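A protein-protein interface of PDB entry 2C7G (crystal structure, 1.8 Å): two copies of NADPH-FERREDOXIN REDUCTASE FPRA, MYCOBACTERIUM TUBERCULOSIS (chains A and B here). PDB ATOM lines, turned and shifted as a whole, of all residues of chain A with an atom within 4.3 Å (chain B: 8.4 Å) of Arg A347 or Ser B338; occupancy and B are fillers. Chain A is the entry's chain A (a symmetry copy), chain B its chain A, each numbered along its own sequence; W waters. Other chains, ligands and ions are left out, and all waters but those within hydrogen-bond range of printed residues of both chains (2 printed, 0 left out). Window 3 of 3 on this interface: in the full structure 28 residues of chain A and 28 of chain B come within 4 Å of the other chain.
No position is printed for both chains.
Of the 12 pairs that touch across the chains among the printed residues, none has its exchanged pair printed and touching as well.
NH2 of Arg A347 is in salt-bridge range of OD2 of Asp B335, 2.8 Å away.
Among the printed residues, merely in contact across the chains: Val A344 with Asp B335 (3.8 Å), Val A344 with Ser B338 (3.8 Å), Val A344 with Thr B340 (3.7 Å), Arg A347 with Gln B337 (3.6 Å), Arg A347 with Ser B338 (3.9 Å), Asn A349 with Phe B334 (3.7 Å), Asn A349 with Asp B335 (3.1 Å), Asn A349 with Pro B342 (3.2 Å), Ser A351 with Gln B337 (3.95 Å), Pro A352 with Gln B337 (3.7 Å) and Asn A385 with Gln B337 (3.8 Å).
Val A344 touches just these residues of chain B: Asp B335 (3.8 Å), Ser B338 (3.8 Å) and Thr B340 (3.7 Å).
No residue of chain B comes within 4 Å of Gly A345.
Gly A346 touches none of the printed residues of chain B.
Arg A347 touches just these residues of chain B: Asp B335, Gln B337 and Ser B338.
Glu A354 touches none of the printed residues of chain B.
Printed residues of chain A within 4 Å of Phe B334: Asn A349 (3.7 Å).
Ser B338 touches just these residues of chain A: Val A344 and Arg A347.
Of the printed residues of chain A, Pro B342 touches Asn A349 (3.2 Å).
Arg B362 touches none of the printed residues of chain A.
The nearest printed residue of chain A that does not touch Phe B334 is Val A344 (7.3 Å).
Water W1 lies within hydrogen-bond range of O of Pro A352 (2.7 Å), NE2 of Gln B337 (2.8 Å) and OD1 of Asn A385 (3.5 Å).
Water W2 bridges OE1 of Gln B337 (3.0 Å) and O of Ser A351 (3.3 Å).
Of the 21 printed residues of chain B, 6 touch a printed residue of chain A.
Along chain B the printed residues that touch a printed residue of chain A span positions 334 to 342.
Of the 12 printed residues of chain A, 6 touch a printed residue of chain B.
Hydrophobic or aromatic side chains of chain A that line the printed part of chain B: Val A344.
Among the printed residues, Asp or Glu carboxylates within 4 Å of a Lys or Arg side-chain nitrogen of the other chain: Arg A347 with Asp B335.
The side-chain carboxylate of Asp B335 is in hydrogen-bond range of the backbone NH of Ser B338 (3.0 Å).
O of Thr B340 sits at hydrogen-bond distance from N of Asp B335 (2.8 Å).
The side-chain hydroxyl of Ser B338 sits at hydrogen-bond distance from the side-chain hydroxyl of Thr B340 (2.7 Å).
NH1 of Arg A347 is in hydrogen-bond range of O of Ser A351, 2.9 Å away.
OE1 of Glu A354 sits at hydrogen-bond distance from OG of Ser A351.
The side-chain amide oxygen of Asn A385 sits at hydrogen-bond distance from the side-chain hydroxyl of Tyr A355 (2.9 Å).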
ATOM      1  N   ASN A 343      28.292  33.909   8.761  1.00  0.00           N
ATOM      2  CA  ASN A 343      29.021  33.085   7.825  1.00  0.00           C
ATOM      3  C   ASN A 343      29.488  31.770   8.440  1.00  0.00           C
ATOM      4  O   ASN A 343      29.655  31.646   9.657  1.00  0.00           O
ATOM      5  CB  ASN A 343      30.215  33.861   7.268  1.00  0.00           C
ATOM      6  CG  ASN A 343      31.295  34.121   8.315  1.00  0.00           C
ATOM      7  OD1 ASN A 343      32.254  33.363   8.420  1.00  0.00           O
ATOM      8  ND2 ASN A 343      31.142  35.196   9.086  1.00  0.00           N
ATOM      9  N   VAL A 344      29.685  30.792   7.576  1.00  0.00           N
ATOM     10  CA  VAL A 344      30.230  29.513   7.989  1.00  0.00           C
ATOM     11  C   VAL A 344      31.537  29.348   7.218  1.00  0.00           C
ATOM     12  O   VAL A 344      31.534  29.160   6.009  1.00  0.00           O
ATOM     13  CB  VAL A 344      29.233  28.352   7.714  1.00  0.00           C
ATOM     14  CG1 VAL A 344      29.794  27.031   8.222  1.00  0.00           C
ATOM     15  CG2 VAL A 344      27.865  28.636   8.348  1.00  0.00           C
ATOM     16  N   GLY A 345      32.653  29.465   7.930  1.00  0.00           N
ATOM     17  CA  GLY A 345      33.970  29.339   7.334  1.00  0.00           C
ATOM     18  C   GLY A 345      34.259  30.417   6.299  1.00  0.00           C
ATOM     19  O   GLY A 345      35.058  30.209   5.394  1.00  0.00           O
ATOM     20  N   GLY A 346      33.579  31.558   6.421  1.00  0.00           N
ATOM     21  CA  GLY A 346      33.760  32.643   5.462  1.00  0.00           C
ATOM     22  C   GLY A 346      32.733  32.642   4.343  1.00  0.00           C
ATOM     23  O   GLY A 346      32.637  33.607   3.591  1.00  0.00           O
ATOM     24  N   ARG A 347      31.972  31.557   4.220  1.00  0.00           N
ATOM     25  CA  ARG A 347      30.849  31.525   3.275  1.00  0.00           C
ATOM     26  C   ARG A 347      29.586  32.117   3.907  1.00  0.00           C
ATOM     27  O   ARG A 347      29.173  31.705   4.999  1.00  0.00           O
ATOM     28  CB  ARG A 347      30.584  30.105   2.762  1.00  0.00           C
ATOM     29  CG  ARG A 347      29.532  30.055   1.626  1.00  0.00           C
ATOM     30  CD  ARG A 347      29.301  28.626   1.103  1.00  0.00           C
ATOM     31  NE  ARG A 347      29.134  27.676   2.203  1.00  0.00           N
ATOM     32  CZ  ARG A 347      28.049  27.607   2.975  1.00  0.00           C
ATOM     33  NH1 ARG A 347      27.030  28.433   2.764  1.00  0.00           N
ATOM     34  NH2 ARG A 347      28.001  26.729   3.974  1.00  0.00           N
ATOM     35  N   ILE A 348      28.968  33.073   3.215  1.00  0.00           N
ATOM     36  CA  ILE A 348      27.762  33.736   3.730  1.00  0.00           C
ATOM     37  C   ILE A 348      26.604  32.772   4.005  1.00  0.00           C
ATOM     38  O   ILE A 348      26.279  31.941   3.178  1.00  0.00           O
ATOM     39  CB  ILE A 348      27.274  34.852   2.772  1.00  0.00           C
ATOM     40  CG1 ILE A 348      28.327  35.973   2.715  1.00  0.00           C
ATOM     41  CG2 ILE A 348      25.891  35.385   3.223  1.00  0.00           C
ATOM     42  CD1 ILE A 348      27.892  37.274   2.054  1.00  0.00           C
ATOM     43  N   ASN A 349      25.965  32.917   5.163  1.00  0.00           N
ATOM     44  CA  ASN A 349      24.843  32.056   5.508  1.00  0.00           C
ATOM     45  C   ASN A 349      23.827  31.939   4.396  1.00  0.00           C
ATOM     46  O   ASN A 349      23.339  32.947   3.886  1.00  0.00           O
ATOM     47  CB  ASN A 349      24.117  32.562   6.753  1.00  0.00           C
ATOM     48  CG  ASN A 349      23.042  31.608   7.204  1.00  0.00           C
ATOM     49  OD1 ASN A 349      21.849  31.868   7.064  1.00  0.00           O
ATOM     50  ND2 ASN A 349      23.461  30.472   7.701  1.00  0.00           N
ATOM     51  N   SER A 351      24.132  30.996   1.369  1.00  0.00           N
ATOM     52  CA  SER A 351      24.633  31.268   0.015  1.00  0.00           C
ATOM     53  C   SER A 351      25.607  30.191  -0.487  1.00  0.00           C
ATOM     54  O   SER A 351      26.488  29.761   0.252  1.00  0.00           O
ATOM     55  CB  SER A 351      25.327  32.639  -0.048  1.00  0.00           C
ATOM     56  OG  SER A 351      25.817  32.895  -1.359  1.00  0.00           O
ATOM     57  N   PRO A 352      25.454  29.748  -1.750  1.00  0.00           N
ATOM     58  CA  PRO A 352      26.435  28.794  -2.264  1.00  0.00           C
ATOM     59  C   PRO A 352      27.727  29.430  -2.795  1.00  0.00           C
ATOM     60  O   PRO A 352      28.736  28.734  -2.936  1.00  0.00           O
ATOM     61  CB  PRO A 352      25.693  28.125  -3.420  1.00  0.00           C
ATOM     62  CG  PRO A 352      24.715  29.142  -3.885  1.00  0.00           C
ATOM     63  CD  PRO A 352      24.386  30.034  -2.726  1.00  0.00           C
ATOM     64  N   GLU A 354      28.690  33.198  -2.179  1.00  0.00           N
ATOM     65  CA  GLU A 354      29.059  34.521  -1.642  1.00  0.00           C
ATOM     66  C   GLU A 354      29.796  34.335  -0.332  1.00  0.00           C
ATOM     67  O   GLU A 354      29.437  33.447   0.466  1.00  0.00           O
ATOM     68  CB  GLU A 354      27.831  35.410  -1.450  1.00  0.00           C
ATOM     69  CG  GLU A 354      27.123  35.750  -2.754  1.00  0.00           C
ATOM     70  CD  GLU A 354      25.675  36.105  -2.533  1.00  0.00           C
ATOM     71  OE1 GLU A 354      24.962  35.317  -1.876  1.00  0.00           O
ATOM     72  OE2 GLU A 354      25.247  37.165  -3.010  1.00  0.00           O
ATOM     73  N   TYR A 355      30.835  35.154  -0.142  1.00  0.00           N
ATOM     74  CA  TYR A 355      31.809  35.009   0.951  1.00  0.00           C
ATOM     75  C   TYR A 355      32.096  36.353   1.608  1.00  0.00           C
ATOM     76  O   TYR A 355      31.760  37.403   1.046  1.00  0.00           O
ATOM     77  CB  TYR A 355      33.133  34.415   0.411  1.00  0.00           C
ATOM     78  CG  TYR A 355      32.940  33.040  -0.164  1.00  0.00           C
ATOM     79  CD1 TYR A 355      32.470  32.871  -1.472  1.00  0.00           C
ATOM     80  CD2 TYR A 355      33.184  31.906   0.607  1.00  0.00           C
ATOM     81  CE1 TYR A 355      32.244  31.594  -2.007  1.00  0.00           C
ATOM     82  CE2 TYR A 355      32.967  30.614   0.080  1.00  0.00           C
ATOM     83  CZ  TYR A 355      32.494  30.481  -1.228  1.00  0.00           C
ATOM     84  OH  TYR A 355      32.278  29.236  -1.755  1.00  0.00           O
ATOM     85  N   ASN A 385      34.831  24.847  -3.008  1.00  0.00           N
ATOM     86  CA  ASN A 385      33.430  24.849  -3.444  1.00  0.00           C
ATOM     87  C   ASN A 385      33.252  24.967  -4.965  1.00  0.00           C
ATOM     88  O   ASN A 385      32.331  24.370  -5.551  1.00  0.00           O
ATOM     89  CB  ASN A 385      32.652  25.973  -2.746  1.00  0.00           C
ATOM     90  CG  ASN A 385      32.392  25.692  -1.266  1.00  0.00           C
ATOM     91  OD1 ASN A 385      32.165  26.617  -0.474  1.00  0.00           O
ATOM     92  ND2 ASN A 385      32.438  24.424  -0.885  1.00  0.00           N
ATOM     93  N   ALA B 106      23.469  16.859  15.390  1.00  0.00           N
ATOM     94  CA  ALA B 106      23.260  16.567  13.971  1.00  0.00           C
ATOM     95  C   ALA B 106      22.392  15.325  13.864  1.00  0.00           C
ATOM     96  O   ALA B 106      22.876  14.199  14.030  1.00  0.00           O
ATOM     97  CB  ALA B 106      24.626  16.355  13.270  1.00  0.00           C
ATOM     98  N   ARG B 110      24.246  12.799   5.869  1.00  0.00           N
ATOM     99  CA  ARG B 110      24.648  13.237   4.535  1.00  0.00           C
ATOM    100  C   ARG B 110      24.381  12.117   3.519  1.00  0.00           C
ATOM    101  O   ARG B 110      24.654  10.934   3.785  1.00  0.00           O
ATOM    102  CB  ARG B 110      26.132  13.606   4.492  1.00  0.00           C
ATOM    103  CG  ARG B 110      26.484  14.853   5.312  1.00  0.00           C
ATOM    104  CD  ARG B 110      27.934  15.306   5.075  1.00  0.00           C
ATOM    105  NE  ARG B 110      28.094  15.901   3.746  1.00  0.00           N
ATOM    106  CZ  ARG B 110      28.692  15.311   2.714  1.00  0.00           C
ATOM    107  NH1 ARG B 110      29.235  14.107   2.845  1.00  0.00           N
ATOM    108  NH2 ARG B 110      28.768  15.941   1.544  1.00  0.00           N
ATOM    109  N   TYR B 324      27.251  12.812   9.558  1.00  0.00           N
ATOM    110  CA  TYR B 324      25.965  13.241  10.096  1.00  0.00           C
ATOM    111  C   TYR B 324      25.646  14.651   9.561  1.00  0.00           C
ATOM    112  O   TYR B 324      26.488  15.301   8.919  1.00  0.00           O
ATOM    113  CB  TYR B 324      26.008  13.206  11.629  1.00  0.00           C
ATOM    114  CG  TYR B 324      25.870  11.816  12.222  1.00  0.00           C
ATOM    115  CD1 TYR B 324      26.733  10.770  11.854  1.00  0.00           C
ATOM    116  CD2 TYR B 324      24.878  11.551  13.175  1.00  0.00           C
ATOM    117  CE1 TYR B 324      26.586   9.481  12.419  1.00  0.00           C
ATOM    118  CE2 TYR B 324      24.718  10.288  13.728  1.00  0.00           C
ATOM    119  CZ  TYR B 324      25.582   9.264  13.363  1.00  0.00           C
ATOM    120  OH  TYR B 324      25.397   8.030  13.933  1.00  0.00           O
ATOM    121  N   ARG B 325      24.436  15.123   9.819  1.00  0.00           N
ATOM    122  CA  ARG B 325      24.001  16.380   9.253  1.00  0.00           C
ATOM    123  C   ARG B 325      22.922  17.008  10.141  1.00  0.00           C
ATOM    124  O   ARG B 325      22.006  16.316  10.576  1.00  0.00           O
ATOM    125  CB  ARG B 325      23.443  16.123   7.848  1.00  0.00           C
ATOM    126  CG  ARG B 325      22.843  17.337   7.240  1.00  0.00           C
ATOM    127  CD  ARG B 325      22.480  17.110   5.805  1.00  0.00           C
ATOM    128  NE  ARG B 325      21.649  18.217   5.354  1.00  0.00           N
ATOM    129  CZ  ARG B 325      22.094  19.417   4.979  1.00  0.00           C
ATOM    130  NH1 ARG B 325      23.401  19.703   4.981  1.00  0.00           N
ATOM    131  NH2 ARG B 325      21.209  20.333   4.587  1.00  0.00           N
ATOM    132  N   GLY B 326      23.043  18.313  10.399  1.00  0.00           N
ATOM    133  CA  GLY B 326      22.063  19.030  11.206  1.00  0.00           C
ATOM    134  C   GLY B 326      20.753  19.183  10.460  1.00  0.00           C
ATOM    135  O   GLY B 326      20.705  19.083   9.228  1.00  0.00           O
ATOM    136  N   VAL B 327      19.688  19.420  11.219  1.00  0.00           N
ATOM    137  CA  VAL B 327      18.336  19.529  10.670  1.00  0.00           C
ATOM    138  C   VAL B 327      17.803  20.898  11.133  1.00  0.00           C
ATOM    139  O   VAL B 327      18.054  21.289  12.270  1.00  0.00           O
ATOM    140  CB  VAL B 327      17.464  18.363  11.201  1.00  0.00           C
ATOM    141  CG1 VAL B 327      15.989  18.561  10.904  1.00  0.00           C
ATOM    142  CG2 VAL B 327      17.923  17.030  10.599  1.00  0.00           C
ATOM    143  N   PHE B 334      19.126  28.951   9.655  1.00  0.00           N
ATOM    144  CA  PHE B 334      19.829  27.704   9.349  1.00  0.00           C
ATOM    145  C   PHE B 334      20.631  27.853   8.056  1.00  0.00           C
ATOM    146  O   PHE B 334      20.205  28.562   7.135  1.00  0.00           O
ATOM    147  CB  PHE B 334      18.814  26.562   9.253  1.00  0.00           C
ATOM    148  CG  PHE B 334      19.424  25.182   9.246  1.00  0.00           C
ATOM    149  CD1 PHE B 334      19.976  24.632  10.413  1.00  0.00           C
ATOM    150  CD2 PHE B 334      19.409  24.417   8.080  1.00  0.00           C
ATOM    151  CE1 PHE B 334      20.515  23.356  10.409  1.00  0.00           C
ATOM    152  CE2 PHE B 334      19.956  23.133   8.066  1.00  0.00           C
ATOM    153  CZ  PHE B 334      20.510  22.606   9.236  1.00  0.00           C
ATOM    154  N   ASP B 335      21.805  27.229   8.017  1.00  0.00           N
ATOM    155  CA  ASP B 335      22.619  27.182   6.814  1.00  0.00           C
ATOM    156  C   ASP B 335      22.487  25.782   6.224  1.00  0.00           C
ATOM    157  O   ASP B 335      23.054  24.824   6.750  1.00  0.00           O
ATOM    158  CB  ASP B 335      24.089  27.504   7.121  1.00  0.00           C
ATOM    159  CG  ASP B 335      24.971  27.440   5.883  1.00  0.00           C
ATOM    160  OD1 ASP B 335      24.756  28.222   4.948  1.00  0.00           O
ATOM    161  OD2 ASP B 335      25.896  26.612   5.855  1.00  0.00           O
ATOM    162  N   ASP B 336      21.728  25.675   5.139  1.00  0.00           N
ATOM    163  CA  ASP B 336      21.423  24.384   4.522  1.00  0.00           C
ATOM    164  C   ASP B 336      22.678  23.617   4.118  1.00  0.00           C
ATOM    165  O   ASP B 336      22.785  22.415   4.360  1.00  0.00           O
ATOM    166  CB  ASP B 336      20.517  24.578   3.300  1.00  0.00           C
ATOM    167  CG  ASP B 336      20.125  23.262   2.638  1.00  0.00           C
ATOM    168  OD1 ASP B 336      19.676  22.340   3.351  1.00  0.00           O
ATOM    169  OD2 ASP B 336      20.249  23.153   1.394  1.00  0.00           O
ATOM    170  N   GLN B 337      23.626  24.312   3.507  1.00  0.00           N
ATOM    171  CA  GLN B 337      24.787  23.639   2.951  1.00  0.00           C
ATOM    172  C   GLN B 337      25.623  22.968   4.045  1.00  0.00           C
ATOM    173  O   GLN B 337      25.996  21.809   3.911  1.00  0.00           O
ATOM    174  CB  GLN B 337      25.613  24.609   2.108  1.00  0.00           C
ATOM    175  CG  GLN B 337      26.825  23.984   1.461  1.00  0.00           C
ATOM    176  CD  GLN B 337      27.515  24.919   0.459  1.00  0.00           C
ATOM    177  OE1 GLN B 337      26.912  25.846  -0.073  1.00  0.00           O
ATOM    178  NE2 GLN B 337      28.782  24.656   0.201  1.00  0.00           N
ATOM    179  N   SER B 338      25.871  23.683   5.139  1.00  0.00           N
ATOM    180  CA  SER B 338      26.665  23.135   6.247  1.00  0.00           C
ATOM    181  C   SER B 338      25.838  22.342   7.273  1.00  0.00           C
ATOM    182  O   SER B 338      26.400  21.570   8.065  1.00  0.00           O
ATOM    183  CB  SER B 338      27.427  24.247   6.949  1.00  0.00           C
ATOM    184  OG  SER B 338      26.527  25.131   7.591  1.00  0.00           O
ATOM    185  N   GLY B 339      24.521  22.546   7.280  1.00  0.00           N
ATOM    186  CA  GLY B 339      23.652  21.941   8.293  1.00  0.00           C
ATOM    187  C   GLY B 339      23.954  22.465   9.694  1.00  0.00           C
ATOM    188  O   GLY B 339      23.907  21.718  10.673  1.00  0.00           O
ATOM    189  N   THR B 340      24.273  23.754   9.780  1.00  0.00           N
ATOM    190  CA  THR B 340      24.560  24.424  11.052  1.00  0.00           C
ATOM    191  C   THR B 340      23.676  25.655  11.229  1.00  0.00           C
ATOM    192  O   THR B 340      23.079  26.137  10.265  1.00  0.00           O
ATOM    193  CB  THR B 340      26.051  24.857  11.174  1.00  0.00           C
ATOM    194  OG1 THR B 340      26.358  25.841  10.172  1.00  0.00           O
ATOM    195  CG2 THR B 340      26.990  23.652  11.024  1.00  0.00           C
ATOM    196  N   ILE B 341      23.586  26.155  12.464  1.00  0.00           N
ATOM    197  CA  ILE B 341      22.853  27.410  12.727  1.00  0.00           C
ATOM    198  C   ILE B 341      23.854  28.561  12.713  1.00  0.00           C
ATOM    199  O   ILE B 341      24.831  28.530  13.482  1.00  0.00           O
ATOM    200  CB  ILE B 341      22.104  27.357  14.093  1.00  0.00           C
ATOM    201  CG1 ILE B 341      21.008  26.295  14.043  1.00  0.00           C
ATOM    202  CG2 ILE B 341      21.492  28.722  14.456  1.00  0.00           C
ATOM    203  CD1 ILE B 341      20.417  25.937  15.415  1.00  0.00           C
ATOM    204  N   PRO B 342      23.640  29.576  11.849  1.00  0.00           N
ATOM    205  CA  PRO B 342      24.639  30.648  11.819  1.00  0.00           C
ATOM    206  C   PRO B 342      24.717  31.374  13.156  1.00  0.00           C
ATOM    207  O   PRO B 342      23.683  31.616  13.814  1.00  0.00           O
ATOM    208  CB  PRO B 342      24.119  31.591  10.726  1.00  0.00           C
ATOM    209  CG  PRO B 342      22.639  31.362  10.708  1.00  0.00           C
ATOM    210  CD  PRO B 342      22.534  29.842  10.907  1.00  0.00           C
ATOM    211  N   TRP B 359      27.679  20.239  17.916  1.00  0.00           N
ATOM    212  CA  TRP B 359      27.702  19.923  16.503  1.00  0.00           C
ATOM    213  C   TRP B 359      26.744  20.756  15.682  1.00  0.00           C
ATOM    214  O   TRP B 359      26.962  20.932  14.497  1.00  0.00           O
ATOM    215  CB  TRP B 359      27.415  18.444  16.309  1.00  0.00           C
ATOM    216  CG  TRP B 359      28.622  17.586  16.498  1.00  0.00           C
ATOM    217  CD1 TRP B 359      29.821  17.934  17.080  1.00  0.00           C
ATOM    218  CD2 TRP B 359      28.748  16.230  16.094  1.00  0.00           C
ATOM    219  NE1 TRP B 359      30.692  16.862  17.044  1.00  0.00           N
ATOM    220  CE2 TRP B 359      30.059  15.807  16.432  1.00  0.00           C
ATOM    221  CE3 TRP B 359      27.888  15.332  15.452  1.00  0.00           C
ATOM    222  CZ2 TRP B 359      30.522  14.513  16.160  1.00  0.00           C
ATOM    223  CZ3 TRP B 359      28.356  14.043  15.171  1.00  0.00           C
ATOM    224  CH2 TRP B 359      29.665  13.651  15.532  1.00  0.00           C
ATOM    225  N   ILE B 360      25.703  21.302  16.307  1.00  0.00           N
ATOM    226  CA  ILE B 360      24.810  22.188  15.543  1.00  0.00           C
ATOM    227  C   ILE B 360      25.493  23.535  15.251  1.00  0.00           C
ATOM    228  O   ILE B 360      25.148  24.215  14.294  1.00  0.00           O
ATOM    229  CB  ILE B 360      23.418  22.365  16.209  1.00  0.00           C
ATOM    230  CG1 ILE B 360      22.416  22.934  15.195  1.00  0.00           C
ATOM    231  CG2 ILE B 360      23.505  23.242  17.456  1.00  0.00           C
ATOM    232  CD1 ILE B 360      22.172  22.042  13.982  1.00  0.00           C
ATOM    233  N   LYS B 361      26.476  23.894  16.075  1.00  0.00           N
ATOM    234  CA  LYS B 361      27.244  25.124  15.887  1.00  0.00           C
ATOM    235  C   LYS B 361      28.448  24.883  14.977  1.00  0.00           C
ATOM    236  O   LYS B 361      28.664  25.631  14.007  1.00  0.00           O
ATOM    237  CB  LYS B 361      27.680  25.630  17.258  1.00  0.00           C
ATOM    238  CG  LYS B 361      28.757  26.735  17.327  1.00  0.00           C
ATOM    239  CD  LYS B 361      29.268  26.728  18.763  1.00  0.00           C
ATOM    240  CE  LYS B 361      29.951  27.993  19.154  1.00  0.00           C
ATOM    241  NZ  LYS B 361      30.351  27.872  20.575  1.00  0.00           N
ATOM    242  N   ARG B 362      29.223  23.847  15.292  1.00  0.00           N
ATOM    243  CA  ARG B 362      30.530  23.619  14.650  1.00  0.00           C
ATOM    244  C   ARG B 362      30.471  22.703  13.423  1.00  0.00           C
ATOM    245  O   ARG B 362      31.421  22.649  12.641  1.00  0.00           O
ATOM    246  CB  ARG B 362      31.521  23.008  15.656  1.00  0.00           C
ATOM    247  CG  ARG B 362      31.762  23.841  16.920  1.00  0.00           C
ATOM    248  CD  ARG B 362      32.906  23.266  17.764  1.00  0.00           C
ATOM    249  NE  ARG B 362      32.493  22.075  18.508  1.00  0.00           N
ATOM    250  CZ  ARG B 362      32.890  20.838  18.235  1.00  0.00           C
ATOM    251  NH1 ARG B 362      33.748  20.611  17.250  1.00  0.00           N
ATOM    252  NH2 ARG B 362      32.448  19.828  18.968  1.00  0.00           N
ATOM    253  N   GLY B 363      29.377  21.967  13.263  1.00  0.00           N
ATOM    254  CA  GLY B 363      29.361  20.857  12.307  1.00  0.00           C
ATOM    255  C   GLY B 363      29.793  19.574  13.012  1.00  0.00           C
ATOM    256  O   GLY B 363      30.340  19.633  14.109  1.00  0.00           O
ATOM    257  N   PRO B 364      29.529  18.412  12.390  1.00  0.00           N
ATOM    258  CA  PRO B 364      29.763  17.105  13.010  1.00  0.00           C
ATOM    259  C   PRO B 364      31.232  16.692  13.073  1.00  0.00           C
ATOM    260  O   PRO B 364      31.625  15.711  12.436  1.00  0.00           O
ATOM    261  CB  PRO B 364      28.954  16.152  12.123  1.00  0.00           C
ATOM    262  CG  PRO B 364      28.945  16.792  10.796  1.00  0.00           C
ATOM    263  CD  PRO B 364      28.925  18.284  11.048  1.00  0.00           C
HETATM  264  O   HOH W   1      29.161  26.129  -2.192  1.00  0.00           O
HETATM  265  O   HOH W   2      24.270  27.322   0.197  1.00  0.00           O
